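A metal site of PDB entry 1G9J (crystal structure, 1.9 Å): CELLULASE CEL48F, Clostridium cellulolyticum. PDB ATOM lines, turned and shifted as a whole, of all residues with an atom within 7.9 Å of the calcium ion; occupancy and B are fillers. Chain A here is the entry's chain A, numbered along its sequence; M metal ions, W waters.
Of the 17 residues printed, 3 come within 4 Å of the calcium ion.
The nearest printed residue that does not touch the calcium ion is Arg 549 (4.3 Å).
The backbone carbonyl oxygen (O) of Gln 185 is bound to the calcium ion (2.3 Å).
Water W2 is bound to the calcium ion, at 2.4 Å.
OE2 of Glu 190 is bound to the calcium ion (2.4 Å).
Water W1 binds the calcium ion, 2.4 Å away.
The calcium ion is bound by the side-chain carboxylate (OD2) of Asp 405, at 2.5 Å.
OE1 of Gln 185 is bound to the calcium ion (2.5 Å).
OE1 of Glu 190 is bound to the calcium ion, 2.6 Å away.
The calcium ion has seven donor atoms within binding distance.
OE2 of Glu 190 lies close to NH2 of Arg 549, 3.3 Å away.
The side-chain carboxylate (OE2) of Glu 190 lies close to the side-chain hydroxyl (OG) of Ser 187, at 2.7 Å.
The guanidinium group (NH1) of Arg 549 lies within salt-bridge range of the side-chain carboxylate (OD1) of Asp 405 (3.1 Å).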
ATOM      1  N   GLN A 116       9.144  14.618  20.240  1.00  0.00           N
ATOM      2  CA  GLN A 116       8.886  16.048  20.332  1.00  0.00           C
ATOM      3  C   GLN A 116       9.102  16.668  21.720  1.00  0.00           C
ATOM      4  O   GLN A 116       8.795  17.828  21.940  1.00  0.00           O
ATOM      5  CB  GLN A 116       7.479  16.349  19.821  1.00  0.00           C
ATOM      6  CG  GLN A 116       7.350  16.268  18.294  1.00  0.00           C
ATOM      7  CD  GLN A 116       7.705  14.899  17.727  1.00  0.00           C
ATOM      8  OE1 GLN A 116       7.018  13.914  17.976  1.00  0.00           O
ATOM      9  NE2 GLN A 116       8.797  14.839  16.965  1.00  0.00           N
ATOM     10  N   ASP A 117       9.644  15.882  22.647  1.00  0.00           N
ATOM     11  CA  ASP A 117       9.935  16.396  23.984  1.00  0.00           C
ATOM     12  C   ASP A 117      11.110  15.595  24.538  1.00  0.00           C
ATOM     13  O   ASP A 117      11.145  14.375  24.424  1.00  0.00           O
ATOM     14  CB  ASP A 117       8.733  16.234  24.914  1.00  0.00           C
ATOM     15  CG  ASP A 117       8.874  17.045  26.183  1.00  0.00           C
ATOM     16  OD1 ASP A 117       8.502  18.236  26.172  1.00  0.00           O
ATOM     17  OD2 ASP A 117       9.381  16.515  27.188  1.00  0.00           O
ATOM     18  N   PRO A 118      12.086  16.282  25.147  1.00  0.00           N
ATOM     19  CA  PRO A 118      13.276  15.623  25.715  1.00  0.00           C
ATOM     20  C   PRO A 118      12.976  14.563  26.772  1.00  0.00           C
ATOM     21  O   PRO A 118      13.789  13.670  27.008  1.00  0.00           O
ATOM     22  CB  PRO A 118      14.075  16.789  26.281  1.00  0.00           C
ATOM     23  CG  PRO A 118      13.696  17.929  25.408  1.00  0.00           C
ATOM     24  CD  PRO A 118      12.201  17.746  25.272  1.00  0.00           C
ATOM     25  N   GLY A 183      15.796  15.787  20.201  1.00  0.00           N
ATOM     26  CA  GLY A 183      14.650  16.354  19.508  1.00  0.00           C
ATOM     27  C   GLY A 183      14.462  17.851  19.368  1.00  0.00           C
ATOM     28  O   GLY A 183      15.170  18.659  19.968  1.00  0.00           O
ATOM     29  N   GLU A 184      13.452  18.207  18.568  1.00  0.00           N
ATOM     30  CA  GLU A 184      13.131  19.595  18.249  1.00  0.00           C
ATOM     31  C   GLU A 184      12.861  20.531  19.417  1.00  0.00           C
ATOM     32  O   GLU A 184      12.904  21.744  19.245  1.00  0.00           O
ATOM     33  CB  GLU A 184      11.947  19.641  17.272  1.00  0.00           C
ATOM     34  CG  GLU A 184      10.662  18.987  17.788  1.00  0.00           C
ATOM     35  CD  GLU A 184       9.482  19.225  16.861  1.00  0.00           C
ATOM     36  OE1 GLU A 184       9.622  19.007  15.640  1.00  0.00           O
ATOM     37  OE2 GLU A 184       8.407  19.620  17.361  1.00  0.00           O
ATOM     38  N   GLN A 185      12.564  19.989  20.589  1.00  0.00           N
ATOM     39  CA  GLN A 185      12.296  20.860  21.734  1.00  0.00           C
ATOM     40  C   GLN A 185      13.492  21.025  22.664  1.00  0.00           C
ATOM     41  O   GLN A 185      13.399  21.745  23.659  1.00  0.00           O
ATOM     42  CB  GLN A 185      11.081  20.362  22.522  1.00  0.00           C
ATOM     43  CG  GLN A 185       9.783  21.094  22.174  1.00  0.00           C
ATOM     44  CD  GLN A 185       9.863  22.589  22.452  1.00  0.00           C
ATOM     45  OE1 GLN A 185      10.511  23.024  23.418  1.00  0.00           O
ATOM     46  NE2 GLN A 185       9.196  23.383  21.623  1.00  0.00           N
ATOM     47  N   GLU A 186      14.598  20.357  22.369  1.00  0.00           N
ATOM     48  CA  GLU A 186      15.763  20.518  23.227  1.00  0.00           C
ATOM     49  C   GLU A 186      16.557  21.724  22.744  1.00  0.00           C
ATOM     50  O   GLU A 186      17.319  21.633  21.780  1.00  0.00           O
ATOM     51  CB  GLU A 186      16.643  19.270  23.196  1.00  0.00           C
ATOM     52  CG  GLU A 186      17.809  19.362  24.169  1.00  0.00           C
ATOM     53  CD  GLU A 186      18.758  18.182  24.081  1.00  0.00           C
ATOM     54  OE1 GLU A 186      19.192  17.860  22.956  1.00  0.00           O
ATOM     55  OE2 GLU A 186      19.067  17.586  25.137  1.00  0.00           O
ATOM     56  N   SER A 187      16.357  22.857  23.406  1.00  0.00           N
ATOM     57  CA  SER A 187      17.077  24.078  23.054  1.00  0.00           C
ATOM     58  C   SER A 187      18.482  24.015  23.626  1.00  0.00           C
ATOM     59  O   SER A 187      18.864  23.044  24.271  1.00  0.00           O
ATOM     60  CB  SER A 187      16.370  25.303  23.647  1.00  0.00           C
ATOM     61  OG  SER A 187      16.489  25.314  25.057  1.00  0.00           O
ATOM     62  N   THR A 188      19.254  25.071  23.389  1.00  0.00           N
ATOM     63  CA  THR A 188      20.607  25.167  23.892  1.00  0.00           C
ATOM     64  C   THR A 188      20.608  25.082  25.411  1.00  0.00           C
ATOM     65  O   THR A 188      21.572  24.612  26.030  1.00  0.00           O
ATOM     66  CB  THR A 188      21.236  26.508  23.466  1.00  0.00           C
ATOM     67  OG1 THR A 188      21.121  26.653  22.041  1.00  0.00           O
ATOM     68  CG2 THR A 188      22.688  26.576  23.867  1.00  0.00           C
ATOM     69  N   TRP A 189      19.509  25.522  26.028  1.00  0.00           N
ATOM     70  CA  TRP A 189      19.390  25.534  27.488  1.00  0.00           C
ATOM     71  C   TRP A 189      19.013  24.191  28.125  1.00  0.00           C
ATOM     72  O   TRP A 189      19.106  24.040  29.347  1.00  0.00           O
ATOM     73  CB  TRP A 189      18.358  26.576  27.920  1.00  0.00           C
ATOM     74  CG  TRP A 189      18.576  27.939  27.361  1.00  0.00           C
ATOM     75  CD1 TRP A 189      18.051  28.459  26.212  1.00  0.00           C
ATOM     76  CD2 TRP A 189      19.411  28.955  27.919  1.00  0.00           C
ATOM     77  NE1 TRP A 189      18.508  29.743  26.023  1.00  0.00           N
ATOM     78  CE2 TRP A 189      19.350  30.064  27.055  1.00  0.00           C
ATOM     79  CE3 TRP A 189      20.216  29.036  29.070  1.00  0.00           C
ATOM     80  CZ2 TRP A 189      20.049  31.254  27.305  1.00  0.00           C
ATOM     81  CZ3 TRP A 189      20.910  30.213  29.317  1.00  0.00           C
ATOM     82  CH2 TRP A 189      20.825  31.307  28.433  1.00  0.00           C
ATOM     83  N   GLU A 190      18.614  23.218  27.312  1.00  0.00           N
ATOM     84  CA  GLU A 190      18.145  21.932  27.824  1.00  0.00           C
ATOM     85  C   GLU A 190      19.009  20.708  27.538  1.00  0.00           C
ATOM     86  O   GLU A 190      18.549  19.574  27.716  1.00  0.00           O
ATOM     87  CB  GLU A 190      16.738  21.684  27.293  1.00  0.00           C
ATOM     88  CG  GLU A 190      15.804  22.814  27.617  1.00  0.00           C
ATOM     89  CD  GLU A 190      14.569  22.816  26.748  1.00  0.00           C
ATOM     90  OE1 GLU A 190      13.630  22.028  27.034  1.00  0.00           O
ATOM     91  OE2 GLU A 190      14.551  23.599  25.789  1.00  0.00           O
ATOM     92  N   ALA A 404      12.286  23.813  17.285  1.00  0.00           N
ATOM     93  CA  ALA A 404      11.204  24.752  17.551  1.00  0.00           C
ATOM     94  C   ALA A 404      11.351  25.615  18.804  1.00  0.00           C
ATOM     95  O   ALA A 404      10.432  26.335  19.152  1.00  0.00           O
ATOM     96  CB  ALA A 404       9.880  23.981  17.633  1.00  0.00           C
ATOM     97  N   ASP A 405      12.494  25.546  19.479  1.00  0.00           N
ATOM     98  CA  ASP A 405      12.711  26.334  20.694  1.00  0.00           C
ATOM     99  C   ASP A 405      13.970  27.206  20.561  1.00  0.00           C
ATOM    100  O   ASP A 405      15.039  26.840  21.060  1.00  0.00           O
ATOM    101  CB  ASP A 405      12.847  25.392  21.888  1.00  0.00           C
ATOM    102  CG  ASP A 405      12.839  26.108  23.232  1.00  0.00           C
ATOM    103  OD1 ASP A 405      12.886  27.355  23.273  1.00  0.00           O
ATOM    104  OD2 ASP A 405      12.794  25.400  24.272  1.00  0.00           O
ATOM    105  N   PRO A 406      13.874  28.361  19.878  1.00  0.00           N
ATOM    106  CA  PRO A 406      12.683  28.899  19.213  1.00  0.00           C
ATOM    107  C   PRO A 406      12.596  28.365  17.782  1.00  0.00           C
ATOM    108  O   PRO A 406      13.437  27.558  17.382  1.00  0.00           O
ATOM    109  CB  PRO A 406      12.940  30.403  19.243  1.00  0.00           C
ATOM    110  CG  PRO A 406      14.409  30.462  18.995  1.00  0.00           C
ATOM    111  CD  PRO A 406      14.963  29.353  19.884  1.00  0.00           C
ATOM    112  N   ARG A 549      16.851  31.811  31.578  1.00  0.00           N
ATOM    113  CA  ARG A 549      16.917  30.356  31.530  1.00  0.00           C
ATOM    114  C   ARG A 549      18.174  29.794  32.205  1.00  0.00           C
ATOM    115  O   ARG A 549      18.249  28.605  32.521  1.00  0.00           O
ATOM    116  CB  ARG A 549      16.800  29.882  30.079  1.00  0.00           C
ATOM    117  CG  ARG A 549      15.488  30.361  29.435  1.00  0.00           C
ATOM    118  CD  ARG A 549      15.289  29.867  28.009  1.00  0.00           C
ATOM    119  NE  ARG A 549      14.846  28.476  27.956  1.00  0.00           N
ATOM    120  CZ  ARG A 549      14.415  27.867  26.858  1.00  0.00           C
ATOM    121  NH1 ARG A 549      14.367  28.540  25.704  1.00  0.00           N
ATOM    122  NH2 ARG A 549      14.016  26.612  26.900  1.00  0.00           N
ATOM    123  N   GLN A 553      15.725  27.235  33.861  1.00  0.00           N
ATOM    124  CA  GLN A 553      15.491  26.134  32.944  1.00  0.00           C
ATOM    125  C   GLN A 553      15.882  24.792  33.551  1.00  0.00           C
ATOM    126  O   GLN A 553      17.046  24.531  33.819  1.00  0.00           O
ATOM    127  CB  GLN A 553      16.287  26.312  31.645  1.00  0.00           C
ATOM    128  CG  GLN A 553      16.069  25.181  30.650  1.00  0.00           C
ATOM    129  CD  GLN A 553      14.633  25.121  30.150  1.00  0.00           C
ATOM    130  OE1 GLN A 553      14.142  26.053  29.527  1.00  0.00           O
ATOM    131  NE2 GLN A 553      13.957  24.013  30.442  1.00  0.00           N
ATOM    132  N   GLU A 554      14.896  23.935  33.764  1.00  0.00           N
ATOM    133  CA  GLU A 554      15.188  22.626  34.304  1.00  0.00           C
ATOM    134  C   GLU A 554      15.718  21.763  33.175  1.00  0.00           C
ATOM    135  O   GLU A 554      15.304  21.895  32.028  1.00  0.00           O
ATOM    136  CB  GLU A 554      13.920  21.986  34.880  1.00  0.00           C
ATOM    137  CG  GLU A 554      14.160  20.619  35.499  1.00  0.00           C
ATOM    138  CD  GLU A 554      12.892  20.006  36.064  1.00  0.00           C
ATOM    139  OE1 GLU A 554      12.179  20.697  36.827  1.00  0.00           O
ATOM    140  OE2 GLU A 554      12.606  18.825  35.745  1.00  0.00           O
HETATM  141 CA    CA M   1      12.314  23.142  25.118  1.00  0.00          CA
HETATM  142  O   HOH W   1      11.233  24.607  26.734  1.00  0.00           O
HETATM  143  O   HOH W   2      10.836  21.476  25.918  1.00  0.00           O
